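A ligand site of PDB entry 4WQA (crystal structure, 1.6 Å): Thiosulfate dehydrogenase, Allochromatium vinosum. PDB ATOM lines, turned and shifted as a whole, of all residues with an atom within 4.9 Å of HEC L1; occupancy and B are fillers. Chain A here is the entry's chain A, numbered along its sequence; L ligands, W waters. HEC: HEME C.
NE2 of His 53 binds FE of HEC L1 (2.1 Å). The side-chain sulfur of Cys 49 is bonded to a carbon (CAB) of HEC L1, at 1.7 Å. The side-chain sulfur (SG) of Cys 52 is bonded to a carbon (CAC) of HEC L1 (1.9 Å). FE of HEC L1 is bound by SD of CSS 96, at 2.3 Å. N of Ile 138 sits at hydrogen-bond distance from O2D of HEC L1, 2.8 Å away.
The backbone NH of Cys 49 is in hydrogen-bond range of the backbone carbonyl oxygen of Leu 32 (3.3 Å). The backbone carbonyl oxygen (O) of Ala 67 sits at hydrogen-bond distance from a ring nitrogen (ND1) of His 53 (2.7 Å). O of CSS 96 lies within hydrogen-bond range of the backbone NH (N) of Leu 101 (3.0 Å). SG of CSS 96 is in hydrogen-bond range of NH1 of Arg 92 (3.2 Å). The side-chain hydroxyl of Ser 100 lies close to SD of CSS 96 (3.7 Å). The backbone NH of Ala 67 is in hydrogen-bond range of the backbone carbonyl oxygen of Gly 137 (2.9 Å). The backbone NH (N) of Cys 49 sits at hydrogen-bond distance from the side-chain hydroxyl (OG1) of Thr 35.
Residues that only touch HEC L1: Leu 32 (3.6 Å), Leu 47 (3.9 Å), Ala 48 (3.7 Å), Phe 69 (3.5 Å), Val 72 (3.8 Å), Phe 76 (3.8 Å), Leu 89 (3.4 Å), Arg 92 (3.2 Å), Ile 93 (3.9 Å), Phe 97 (3.4 Å), Ser 100 (3.3 Å), Leu 101 (3.5 Å), Met 120 (3.9 Å), Gly 137 (3.3 Å), Phe 189 (3.7 Å), Met 195 (3.9 Å) and Thr 200 (3.6 Å).
Water W3 bridges an oxygen (O2A) of HEC L1 and the side-chain amide oxygen of Gln 78. Water W4 lies within hydrogen-bond range of an oxygen (O2A) of HEC L1, the side-chain amide nitrogen (NE2) of Gln 78 and the guanidinium group (NE) of Arg 92. Water W7 lies within hydrogen-bond range of O of Pro 68 (2.7 Å), N of Gly 137 (2.7 Å) and O1A of HEC L1 (2.8 Å). Water W2 bridges an oxygen (O1D) of HEC L1 (2.8 Å) and the guanidinium group (NH2) of Arg 92 (3.2 Å). Water W8 lies within hydrogen-bond range of N of Met 195, OG of Ser 100 and N of Gly 194. Water W1 lies within hydrogen-bond range of O of Ile 138 (2.8 Å), OG1 of Thr 200 (3.2 Å) and O2D of HEC L1 (3.4 Å).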
ATOM      1  N   LEU A  32     -13.622  15.012 -16.175  1.00  0.00           N
ATOM      2  CA  LEU A  32     -14.160  13.838 -16.852  1.00  0.00           C
ATOM      3  C   LEU A  32     -15.544  13.454 -16.304  1.00  0.00           C
ATOM      4  O   LEU A  32     -16.351  12.889 -17.034  1.00  0.00           O
ATOM      5  CB  LEU A  32     -13.195  12.671 -16.698  1.00  0.00           C
ATOM      6  CG  LEU A  32     -11.852  12.933 -17.381  1.00  0.00           C
ATOM      7  CD1 LEU A  32     -10.785  11.947 -16.884  1.00  0.00           C
ATOM      8  CD2 LEU A  32     -11.987  12.890 -18.888  1.00  0.00           C
ATOM      9  N   THR A  35     -18.270  17.226 -16.923  1.00  0.00           N
ATOM     10  CA  THR A  35     -17.727  18.032 -18.011  1.00  0.00           C
ATOM     11  C   THR A  35     -18.563  19.230 -18.438  1.00  0.00           C
ATOM     12  O   THR A  35     -18.039  20.334 -18.587  1.00  0.00           O
ATOM     13  CB  THR A  35     -17.473  17.169 -19.260  1.00  0.00           C
ATOM     14  OG1 THR A  35     -17.132  15.848 -18.826  1.00  0.00           O
ATOM     15  CG2 THR A  35     -16.350  17.745 -20.043  1.00  0.00           C
ATOM     16  N   LEU A  47     -23.786  15.651 -21.995  1.00  0.00           N
ATOM     17  CA  LEU A  47     -22.970  14.497 -21.656  1.00  0.00           C
ATOM     18  C   LEU A  47     -21.666  14.874 -21.007  1.00  0.00           C
ATOM     19  O   LEU A  47     -21.053  15.858 -21.386  1.00  0.00           O
ATOM     20  CB  LEU A  47     -22.684  13.670 -22.920  1.00  0.00           C
ATOM     21  CG  LEU A  47     -23.937  13.192 -23.664  1.00  0.00           C
ATOM     22  CD1 LEU A  47     -23.528  12.222 -24.749  1.00  0.00           C
ATOM     23  CD2 LEU A  47     -24.989  12.551 -22.699  1.00  0.00           C
ATOM     24  N   ALA A  48     -21.285  14.099 -20.010  1.00  0.00           N
ATOM     25  CA  ALA A  48     -19.961  14.115 -19.436  1.00  0.00           C
ATOM     26  C   ALA A  48     -19.227  12.905 -19.973  1.00  0.00           C
ATOM     27  O   ALA A  48     -19.845  11.952 -20.453  1.00  0.00           O
ATOM     28  CB  ALA A  48     -20.001  14.092 -17.915  1.00  0.00           C
ATOM     29  N   CYS A  49     -17.897  12.922 -19.898  1.00  0.00           N
ATOM     30  CA  CYS A  49     -17.140  11.787 -20.388  1.00  0.00           C
ATOM     31  C   CYS A  49     -17.572  10.477 -19.720  1.00  0.00           C
ATOM     32  O   CYS A  49     -17.626   9.447 -20.355  1.00  0.00           O
ATOM     33  CB  CYS A  49     -15.632  12.012 -20.172  1.00  0.00           C
ATOM     34  SG  CYS A  49     -15.039  13.614 -20.753  1.00  0.00           S
ATOM     35  N   CYS A  52     -20.230   7.543 -21.069  1.00  0.00           N
ATOM     36  CA  CYS A  52     -19.839   6.392 -21.903  1.00  0.00           C
ATOM     37  C   CYS A  52     -18.570   5.701 -21.433  1.00  0.00           C
ATOM     38  O   CYS A  52     -18.240   4.610 -21.894  1.00  0.00           O
ATOM     39  CB  CYS A  52     -19.639   6.838 -23.350  1.00  0.00           C
ATOM     40  SG  CYS A  52     -21.136   7.595 -24.073  1.00  0.00           S
ATOM     41  N   HIS A  53     -17.861   6.364 -20.516  1.00  0.00           N
ATOM     42  CA  HIS A  53     -16.677   5.822 -19.901  1.00  0.00           C
ATOM     43  C   HIS A  53     -16.881   5.695 -18.383  1.00  0.00           C
ATOM     44  O   HIS A  53     -16.226   6.374 -17.613  1.00  0.00           O
ATOM     45  CB  HIS A  53     -15.494   6.731 -20.194  1.00  0.00           C
ATOM     46  CG  HIS A  53     -15.186   6.903 -21.655  1.00  0.00           C
ATOM     47  ND1 HIS A  53     -14.406   6.003 -22.357  1.00  0.00           N
ATOM     48  CD2 HIS A  53     -15.529   7.858 -22.538  1.00  0.00           C
ATOM     49  CE1 HIS A  53     -14.293   6.403 -23.612  1.00  0.00           C
ATOM     50  NE2 HIS A  53     -14.945   7.537 -23.754  1.00  0.00           N
ATOM     51  N   ALA A  67     -14.733   1.192 -22.676  1.00  0.00           N
ATOM     52  CA  ALA A  67     -13.627   2.073 -23.031  1.00  0.00           C
ATOM     53  C   ALA A  67     -12.916   2.651 -21.815  1.00  0.00           C
ATOM     54  O   ALA A  67     -12.866   3.862 -21.658  1.00  0.00           O
ATOM     55  CB  ALA A  67     -14.120   3.206 -23.910  1.00  0.00           C
ATOM     56  N   PRO A  68     -12.327   1.785 -20.984  1.00  0.00           N
ATOM     57  CA  PRO A  68     -11.539   2.306 -19.857  1.00  0.00           C
ATOM     58  C   PRO A  68     -10.333   3.112 -20.308  1.00  0.00           C
ATOM     59  O   PRO A  68      -9.762   2.869 -21.379  1.00  0.00           O
ATOM     60  CB  PRO A  68     -11.121   1.034 -19.130  1.00  0.00           C
ATOM     61  CG  PRO A  68     -11.144  -0.028 -20.158  1.00  0.00           C
ATOM     62  CD  PRO A  68     -12.222   0.329 -21.122  1.00  0.00           C
ATOM     63  N   PHE A  69      -9.976   4.078 -19.482  1.00  0.00           N
ATOM     64  CA  PHE A  69      -8.782   4.884 -19.711  1.00  0.00           C
ATOM     65  C   PHE A  69      -7.544   4.237 -19.108  1.00  0.00           C
ATOM     66  O   PHE A  69      -6.408   4.718 -19.335  1.00  0.00           O
ATOM     67  CB  PHE A  69      -8.957   6.266 -19.115  1.00  0.00           C
ATOM     68  CG  PHE A  69     -10.087   7.063 -19.705  1.00  0.00           C
ATOM     69  CD1 PHE A  69     -10.386   7.005 -21.055  1.00  0.00           C
ATOM     70  CD2 PHE A  69     -10.846   7.897 -18.890  1.00  0.00           C
ATOM     71  CE1 PHE A  69     -11.420   7.765 -21.588  1.00  0.00           C
ATOM     72  CE2 PHE A  69     -11.878   8.648 -19.418  1.00  0.00           C
ATOM     73  CZ  PHE A  69     -12.167   8.578 -20.776  1.00  0.00           C
ATOM     74  N   VAL A  72      -4.544   3.697 -21.534  1.00  0.00           N
ATOM     75  CA  VAL A  72      -4.769   4.385 -22.804  1.00  0.00           C
ATOM     76  C   VAL A  72      -3.564   5.235 -23.232  1.00  0.00           C
ATOM     77  O   VAL A  72      -3.308   5.365 -24.417  1.00  0.00           O
ATOM     78  CB  VAL A  72      -6.044   5.267 -22.753  1.00  0.00           C
ATOM     79  CG1 VAL A  72      -5.846   6.501 -21.946  1.00  0.00           C
ATOM     80  CG2 VAL A  72      -6.463   5.640 -24.160  1.00  0.00           C
ATOM     81  N   PHE A  76      -0.975   5.765 -27.546  1.00  0.00           N
ATOM     82  CA  PHE A  76      -0.845   6.939 -28.390  1.00  0.00           C
ATOM     83  C   PHE A  76       0.620   7.397 -28.430  1.00  0.00           C
ATOM     84  O   PHE A  76       1.351   7.226 -27.449  1.00  0.00           O
ATOM     85  CB  PHE A  76      -1.739   8.064 -27.867  1.00  0.00           C
ATOM     86  CG  PHE A  76      -3.202   7.814 -28.159  1.00  0.00           C
ATOM     87  CD1 PHE A  76      -3.962   7.013 -27.317  1.00  0.00           C
ATOM     88  CD2 PHE A  76      -3.787   8.337 -29.302  1.00  0.00           C
ATOM     89  CE1 PHE A  76      -5.292   6.749 -27.595  1.00  0.00           C
ATOM     90  CE2 PHE A  76      -5.152   8.068 -29.593  1.00  0.00           C
ATOM     91  CZ  PHE A  76      -5.890   7.279 -28.739  1.00  0.00           C
ATOM     92  N   GLN A  78      -1.064   7.111 -32.351  1.00  0.00           N
ATOM     93  CA  GLN A  78      -1.581   6.000 -33.147  1.00  0.00           C
ATOM     94  C   GLN A  78      -2.282   6.544 -34.393  1.00  0.00           C
ATOM     95  O   GLN A  78      -2.732   7.701 -34.439  1.00  0.00           O
ATOM     96  CB  GLN A  78      -2.556   5.159 -32.309  1.00  0.00           C
ATOM     97  CG  GLN A  78      -3.889   5.888 -32.094  1.00  0.00           C
ATOM     98  CD  GLN A  78      -4.851   5.121 -31.206  1.00  0.00           C
ATOM     99  OE1 GLN A  78      -4.456   4.425 -30.266  1.00  0.00           O
ATOM    100  NE2 GLN A  78      -6.129   5.280 -31.491  1.00  0.00           N
ATOM    101  N   LEU A  89      -3.004  11.579 -28.012  1.00  0.00           N
ATOM    102  CA  LEU A  89      -4.131  11.416 -27.104  1.00  0.00           C
ATOM    103  C   LEU A  89      -4.881  12.755 -26.933  1.00  0.00           C
ATOM    104  O   LEU A  89      -6.131  12.792 -26.846  1.00  0.00           O
ATOM    105  CB  LEU A  89      -3.649  10.863 -25.751  1.00  0.00           C
ATOM    106  CG  LEU A  89      -4.668  10.714 -24.642  1.00  0.00           C
ATOM    107  CD1 LEU A  89      -5.894   9.893 -25.091  1.00  0.00           C
ATOM    108  CD2 LEU A  89      -4.062  10.022 -23.435  1.00  0.00           C
ATOM    109  N   ARG A  92      -7.209  12.991 -29.826  1.00  0.00           N
ATOM    110  CA  ARG A  92      -8.327  12.070 -29.643  1.00  0.00           C
ATOM    111  C   ARG A  92      -9.339  12.686 -28.682  1.00  0.00           C
ATOM    112  O   ARG A  92     -10.537  12.680 -28.953  1.00  0.00           O
ATOM    113  CB  ARG A  92      -7.813  10.740 -29.090  1.00  0.00           C
ATOM    114  CG  ARG A  92      -8.855   9.667 -28.863  1.00  0.00           C
ATOM    115  CD  ARG A  92      -9.346   9.157 -30.231  1.00  0.00           C
ATOM    116  NE  ARG A  92     -10.435   8.201 -30.185  1.00  0.00           N
ATOM    117  CZ  ARG A  92     -11.714   8.537 -30.127  1.00  0.00           C
ATOM    118  NH1 ARG A  92     -12.058   9.816 -30.029  1.00  0.00           N
ATOM    119  NH2 ARG A  92     -12.654   7.607 -30.137  1.00  0.00           N
ATOM    120  N   ILE A  93      -8.872  13.226 -27.569  1.00  0.00           N
ATOM    121  CA  ILE A  93      -9.790  13.846 -26.606  1.00  0.00           C
ATOM    122  C   ILE A  93     -10.545  14.994 -27.255  1.00  0.00           C
ATOM    123  O   ILE A  93     -11.742  15.159 -27.029  1.00  0.00           O
ATOM    124  CB  ILE A  93      -9.054  14.337 -25.348  1.00  0.00           C
ATOM    125  CG1 ILE A  93      -8.598  13.131 -24.526  1.00  0.00           C
ATOM    126  CG2 ILE A  93      -9.978  15.260 -24.513  1.00  0.00           C
ATOM    127  CD1 ILE A  93      -7.639  13.460 -23.377  1.00  0.00           C
ATOM    128  N   CSS A  96     -13.432  13.778 -29.181  1.00  0.00           N
ATOM    129  CA  CSS A  96     -14.507  13.401 -28.273  1.00  0.00           C
ATOM    130  CB  CSS A  96     -14.044  12.680 -26.998  1.00  0.00           C
ATOM    131  SG  CSS A  96     -13.174  11.188 -27.343  1.00  0.00           S
ATOM    132  SD  CSS A  96     -14.798   9.897 -27.469  1.00  0.00           S
ATOM    133  C   CSS A  96     -15.342  14.631 -27.899  1.00  0.00           C
ATOM    134  O   CSS A  96     -16.589  14.587 -27.769  1.00  0.00           O
ATOM    135  N   PHE A  97     -14.643  15.756 -27.678  1.00  0.00           N
ATOM    136  CA  PHE A  97     -15.334  17.001 -27.307  1.00  0.00           C
ATOM    137  C   PHE A  97     -16.191  17.441 -28.488  1.00  0.00           C
ATOM    138  O   PHE A  97     -17.314  17.910 -28.291  1.00  0.00           O
ATOM    139  CB  PHE A  97     -14.367  18.120 -26.920  1.00  0.00           C
ATOM    140  CG  PHE A  97     -14.076  18.194 -25.438  1.00  0.00           C
ATOM    141  CD1 PHE A  97     -13.038  17.457 -24.884  1.00  0.00           C
ATOM    142  CD2 PHE A  97     -14.834  19.009 -24.590  1.00  0.00           C
ATOM    143  CE1 PHE A  97     -12.763  17.516 -23.541  1.00  0.00           C
ATOM    144  CE2 PHE A  97     -14.568  19.081 -23.241  1.00  0.00           C
ATOM    145  CZ  PHE A  97     -13.518  18.346 -22.714  1.00  0.00           C
ATOM    146  N   SER A 100     -18.790  13.372 -29.422  1.00  0.00           N
ATOM    147  CA  SER A 100     -19.591  12.856 -28.321  1.00  0.00           C
ATOM    148  C   SER A 100     -20.211  13.929 -27.445  1.00  0.00           C
ATOM    149  O   SER A 100     -21.350  13.752 -26.966  1.00  0.00           O
ATOM    150  CB  SER A 100     -18.731  11.946 -27.477  1.00  0.00           C
ATOM    151  OG  SER A 100     -18.359  10.796 -28.226  1.00  0.00           O
ATOM    152  N   LEU A 101     -19.508  15.041 -27.254  1.00  0.00           N
ATOM    153  CA  LEU A 101     -20.006  16.159 -26.449  1.00  0.00           C
ATOM    154  C   LEU A 101     -20.491  17.352 -27.304  1.00  0.00           C
ATOM    155  O   LEU A 101     -20.826  18.410 -26.767  1.00  0.00           O
ATOM    156  CB  LEU A 101     -18.944  16.676 -25.468  1.00  0.00           C
ATOM    157  CG  LEU A 101     -18.251  15.723 -24.497  1.00  0.00           C
ATOM    158  CD1 LEU A 101     -17.724  16.483 -23.248  1.00  0.00           C
ATOM    159  CD2 LEU A 101     -19.151  14.649 -24.068  1.00  0.00           C
ATOM    160  N   MET A 116      -6.814  16.296 -17.490  1.00  0.00           N
ATOM    161  CA  MET A 116      -7.380  15.035 -17.976  1.00  0.00           C
ATOM    162  C   MET A 116      -6.309  14.014 -18.338  1.00  0.00           C
ATOM    163  O   MET A 116      -6.413  12.853 -17.957  1.00  0.00           O
ATOM    164  CB  MET A 116      -8.318  15.288 -19.166  1.00  0.00           C
ATOM    165  CG  MET A 116      -9.558  16.027 -18.768  1.00  0.00           C
ATOM    166  SD  MET A 116     -10.707  16.180 -20.161  1.00  0.00           S
ATOM    167  CE  MET A 116     -10.441  17.876 -20.668  1.00  0.00           C
ATOM    168  N   MET A 120      -5.621  10.326 -16.723  1.00  0.00           N
ATOM    169  CA  MET A 120      -5.467   9.101 -17.503  1.00  0.00           C
ATOM    170  C   MET A 120      -4.096   8.427 -17.294  1.00  0.00           C
ATOM    171  O   MET A 120      -4.004   7.202 -17.253  1.00  0.00           O
ATOM    172  CB  MET A 120      -5.690   9.394 -19.000  1.00  0.00           C
ATOM    173  CG  MET A 120      -7.092   9.838 -19.287  1.00  0.00           C
ATOM    174  SD  MET A 120      -7.320  10.065 -21.059  1.00  0.00           S
ATOM    175  CE  MET A 120      -8.977  10.755 -21.045  1.00  0.00           C
ATOM    176  N   GLY A 137     -11.348  -0.489 -24.797  1.00  0.00           N
ATOM    177  CA  GLY A 137     -12.295  -0.167 -25.838  1.00  0.00           C
ATOM    178  C   GLY A 137     -13.728  -0.618 -25.566  1.00  0.00           C
ATOM    179  O   GLY A 137     -14.095  -1.020 -24.432  1.00  0.00           O
ATOM    180  N   ILE A 138     -14.521  -0.523 -26.621  1.00  0.00           N
ATOM    181  CA  ILE A 138     -15.904  -1.014 -26.604  1.00  0.00           C
ATOM    182  C   ILE A 138     -15.996  -2.093 -27.700  1.00  0.00           C
ATOM    183  O   ILE A 138     -15.958  -1.777 -28.894  1.00  0.00           O
ATOM    184  CB  ILE A 138     -16.903   0.128 -26.817  1.00  0.00           C
ATOM    185  CG1 ILE A 138     -16.935   0.999 -25.560  1.00  0.00           C
ATOM    186  CG2 ILE A 138     -18.331  -0.403 -27.093  1.00  0.00           C
ATOM    187  CD1 ILE A 138     -17.500   2.350 -25.803  1.00  0.00           C
ATOM    188  N   PHE A 189     -25.330  12.810 -27.905  1.00  0.00           N
ATOM    189  CA  PHE A 189     -24.174  12.823 -28.783  1.00  0.00           C
ATOM    190  C   PHE A 189     -24.605  13.140 -30.228  1.00  0.00           C
ATOM    191  O   PHE A 189     -25.766  12.887 -30.604  1.00  0.00           O
ATOM    192  CB  PHE A 189     -23.416  11.473 -28.674  1.00  0.00           C
ATOM    193  CG  PHE A 189     -24.222  10.240 -29.033  1.00  0.00           C
ATOM    194  CD1 PHE A 189     -24.382   9.844 -30.357  1.00  0.00           C
ATOM    195  CD2 PHE A 189     -24.793   9.468 -28.026  1.00  0.00           C
ATOM    196  CE1 PHE A 189     -25.101   8.718 -30.687  1.00  0.00           C
ATOM    197  CE2 PHE A 189     -25.511   8.310 -28.329  1.00  0.00           C
ATOM    198  CZ  PHE A 189     -25.672   7.946 -29.681  1.00  0.00           C
ATOM    199  N   GLY A 194     -18.765   8.042 -32.212  1.00  0.00           N
ATOM    200  CA  GLY A 194     -18.662   6.600 -32.391  1.00  0.00           C
ATOM    201  C   GLY A 194     -19.916   5.883 -31.920  1.00  0.00           C
ATOM    202  O   GLY A 194     -20.265   4.819 -32.430  1.00  0.00           O
ATOM    203  N   MET A 195     -20.600   6.454 -30.933  1.00  0.00           N
ATOM    204  CA  MET A 195     -21.784   5.795 -30.405  1.00  0.00           C
ATOM    205  C   MET A 195     -22.932   5.827 -31.410  1.00  0.00           C
ATOM    206  O   MET A 195     -23.916   5.119 -31.242  1.00  0.00           O
ATOM    207  CB  MET A 195     -22.179   6.448 -29.059  1.00  0.00           C
ATOM    208  CG  MET A 195     -23.149   5.635 -28.261  1.00  0.00           C
ATOM    209  SD  MET A 195     -22.534   4.030 -27.672  1.00  0.00           S
ATOM    210  CE  MET A 195     -21.328   4.510 -26.424  1.00  0.00           C
ATOM    211  N   THR A 200     -21.126  -0.438 -32.560  1.00  0.00           N
ATOM    212  CA  THR A 200     -20.527   0.119 -31.345  1.00  0.00           C
ATOM    213  C   THR A 200     -21.621   0.326 -30.285  1.00  0.00           C
ATOM    214  O   THR A 200     -21.448  -0.079 -29.133  1.00  0.00           O
ATOM    215  CB  THR A 200     -19.769   1.439 -31.634  1.00  0.00           C
ATOM    216  OG1 THR A 200     -18.660   1.183 -32.520  1.00  0.00           O
ATOM    217  CG2 THR A 200     -19.233   2.072 -30.342  1.00  0.00           C
HETATM  218 FE   HEC L   1     -14.830   8.720 -25.500  1.00  0.00          FE
HETATM  219  CHA HEC L   1     -12.937   6.343 -27.205  1.00  0.00           C
HETATM  220  CHB HEC L   1     -11.919  10.077 -24.197  1.00  0.00           C
HETATM  221  CHC HEC L   1     -16.689  11.217 -24.063  1.00  0.00           C
HETATM  222  CHD HEC L   1     -17.767   7.103 -26.543  1.00  0.00           C
HETATM  223  NA  HEC L   1     -12.810   8.290 -25.659  1.00  0.00           N
HETATM  224  C1A HEC L   1     -12.276   7.315 -26.375  1.00  0.00           C
HETATM  225  C2A HEC L   1     -10.800   7.272 -26.297  1.00  0.00           C
HETATM  226  C3A HEC L   1     -10.499   8.369 -25.380  1.00  0.00           C
HETATM  227  C4A HEC L   1     -11.810   8.924 -25.063  1.00  0.00           C
HETATM  228  CMA HEC L   1      -9.170   8.852 -24.885  1.00  0.00           C
HETATM  229  CAA HEC L   1      -9.886   6.277 -26.941  1.00  0.00           C
HETATM  230  CBA HEC L   1      -9.926   5.021 -26.083  1.00  0.00           C
HETATM  231  CGA HEC L   1      -8.914   3.993 -26.545  1.00  0.00           C
HETATM  232  O1A HEC L   1      -8.788   2.906 -25.904  1.00  0.00           O
HETATM  233  O2A HEC L   1      -8.206   4.256 -27.547  1.00  0.00           O
HETATM  234  NB  HEC L   1     -14.387  10.349 -24.368  1.00  0.00           N
HETATM  235  C1B HEC L   1     -13.183  10.711 -23.933  1.00  0.00           C
HETATM  236  C2B HEC L   1     -13.229  11.951 -23.137  1.00  0.00           C
HETATM  237  C3B HEC L   1     -14.629  12.306 -23.087  1.00  0.00           C
HETATM  238  C4B HEC L   1     -15.250  11.226 -23.902  1.00  0.00           C
HETATM  239  CMB HEC L   1     -12.109  12.656 -22.488  1.00  0.00           C
HETATM  240  CAB HEC L   1     -15.265  13.498 -22.433  1.00  0.00           C
HETATM  241  CBB HEC L   1     -14.742  14.739 -23.151  1.00  0.00           C
HETATM  242  NC  HEC L   1     -16.854   9.086 -25.352  1.00  0.00           N
HETATM  243  C1C HEC L   1     -17.384  10.130 -24.732  1.00  0.00           C
HETATM  244  C2C HEC L   1     -18.881  10.093 -24.705  1.00  0.00           C
HETATM  245  C3C HEC L   1     -19.191   8.879 -25.453  1.00  0.00           C
HETATM  246  C4C HEC L   1     -17.865   8.331 -25.788  1.00  0.00           C
HETATM  247  CMC HEC L   1     -19.830  11.082 -24.074  1.00  0.00           C
HETATM  248  CAC HEC L   1     -20.537   8.270 -25.772  1.00  0.00           C
HETATM  249  CBC HEC L   1     -21.505   9.240 -26.408  1.00  0.00           C
HETATM  250  ND  HEC L   1     -15.248   7.048 -26.638  1.00  0.00           N
HETATM  251  C1D HEC L   1     -16.461   6.598 -26.966  1.00  0.00           C
HETATM  252  C2D HEC L   1     -16.408   5.396 -27.830  1.00  0.00           C
HETATM  253  C3D HEC L   1     -14.997   5.162 -28.039  1.00  0.00           C
HETATM  254  C4D HEC L   1     -14.370   6.270 -27.264  1.00  0.00           C
HETATM  255  CMD HEC L   1     -17.573   4.612 -28.380  1.00  0.00           C
HETATM  256  CAD HEC L   1     -14.384   4.073 -28.871  1.00  0.00           C
HETATM  257  CBD HEC L   1     -13.965   2.880 -28.026  1.00  0.00           C
HETATM  258  CGD HEC L   1     -13.060   1.950 -28.818  1.00  0.00           C
HETATM  259  O1D HEC L   1     -12.052   2.467 -29.373  1.00  0.00           O
HETATM  260  O2D HEC L   1     -13.310   0.719 -28.877  1.00  0.00           O
HETATM  261 FE   HEC L   2     -28.370   3.301 -20.208  1.00  0.00          FE
HETATM  262  CHA HEC L   2     -25.491   5.173 -20.433  1.00  0.00           C
HETATM  263  CHB HEC L   2     -28.467   2.901 -23.619  1.00  0.00           C
HETATM  264  CHC HEC L   2     -30.931   0.944 -19.844  1.00  0.00           C
HETATM  265  CHD HEC L   2     -28.721   4.155 -16.855  1.00  0.00           C
HETATM  266  NA  HEC L   2     -27.202   3.937 -21.771  1.00  0.00           N
HETATM  267  C1A HEC L   2     -26.103   4.685 -21.661  1.00  0.00           C
HETATM  268  C2A HEC L   2     -25.531   5.005 -22.966  1.00  0.00           C
HETATM  269  C3A HEC L   2     -26.408   4.320 -23.929  1.00  0.00           C
HETATM  270  C4A HEC L   2     -27.414   3.710 -23.048  1.00  0.00           C
HETATM  271  CMA HEC L   2     -26.275   4.283 -25.414  1.00  0.00           C
HETATM  272  CAA HEC L   2     -24.330   5.818 -23.281  1.00  0.00           C
HETATM  273  CBA HEC L   2     -24.633   7.293 -22.940  1.00  0.00           C
HETATM  274  CGA HEC L   2     -25.611   8.088 -23.814  1.00  0.00           C
HETATM  275  O1A HEC L   2     -26.219   9.054 -23.286  1.00  0.00           O
HETATM  276  O2A HEC L   2     -25.788   7.824 -25.020  1.00  0.00           O
HETATM  277  NB  HEC L   2     -29.463   2.133 -21.478  1.00  0.00           N
HETATM  278  C1B HEC L   2     -29.362   2.135 -22.792  1.00  0.00           C
HETATM  279  C2B HEC L   2     -30.290   1.181 -23.404  1.00  0.00           C
HETATM  280  C3B HEC L   2     -31.004   0.591 -22.293  1.00  0.00           C
HETATM  281  C4B HEC L   2     -30.405   1.244 -21.140  1.00  0.00           C
HETATM  282  CMB HEC L   2     -30.483   0.854 -24.850  1.00  0.00           C
HETATM  283  CAB HEC L   2     -32.073  -0.461 -22.338  1.00  0.00           C
HETATM  284  CBB HEC L   2     -31.433  -1.748 -22.838  1.00  0.00           C
HETATM  285  NC  HEC L   2     -29.604   2.679 -18.649  1.00  0.00           N
HETATM  286  C1C HEC L   2     -30.542   1.745 -18.692  1.00  0.00           C
HETATM  287  C2C HEC L   2     -31.287   1.595 -17.432  1.00  0.00           C
HETATM  288  C3C HEC L   2     -30.668   2.552 -16.539  1.00  0.00           C
HETATM  289  C4C HEC L   2     -29.625   3.159 -17.403  1.00  0.00           C
HETATM  290  CMC HEC L   2     -32.428   0.648 -17.195  1.00  0.00           C
HETATM  291  CAC HEC L   2     -31.016   2.894 -15.105  1.00  0.00           C
HETATM  292  CBC HEC L   2     -31.015   1.750 -14.155  1.00  0.00           C
HETATM  293  ND  HEC L   2     -27.284   4.450 -18.902  1.00  0.00           N
HETATM  294  C1D HEC L   2     -27.565   4.640 -17.608  1.00  0.00           C
HETATM  295  C2D HEC L   2     -26.513   5.466 -16.953  1.00  0.00           C
HETATM  296  C3D HEC L   2     -25.563   5.759 -18.010  1.00  0.00           C
HETATM  297  C4D HEC L   2     -26.145   5.049 -19.170  1.00  0.00           C
HETATM  298  CMD HEC L   2     -26.449   5.902 -15.539  1.00  0.00           C
HETATM  299  CAD HEC L   2     -24.265   6.531 -17.965  1.00  0.00           C
HETATM  300  CBD HEC L   2     -23.138   5.459 -17.895  1.00  0.00           C
HETATM  301  CGD HEC L   2     -23.035   4.678 -16.584  1.00  0.00           C
HETATM  302  O1D HEC L   2     -23.178   3.425 -16.607  1.00  0.00           O
HETATM  303  O2D HEC L   2     -22.794   5.277 -15.502  1.00  0.00           O
HETATM  304  O   HOH W   1     -16.255   0.413 -30.590  1.00  0.00           O
HETATM  305  O   HOH W   2     -11.051   4.854 -30.529  1.00  0.00           O
HETATM  306  O   HOH W   3      -6.348   2.689 -28.666  1.00  0.00           O
HETATM  307  O   HOH W   4      -8.557   5.412 -29.957  1.00  0.00           O
HETATM  308  O   HOH W   5      -8.994   0.545 -27.383  1.00  0.00           O
HETATM  309  O   HOH W   6      -6.720   1.730 -24.148  1.00  0.00           O
HETATM  310  O   HOH W   7     -10.321   1.884 -23.862  1.00  0.00           O
HETATM  311  O   HOH W   8     -19.048   8.095 -29.135  1.00  0.00           O
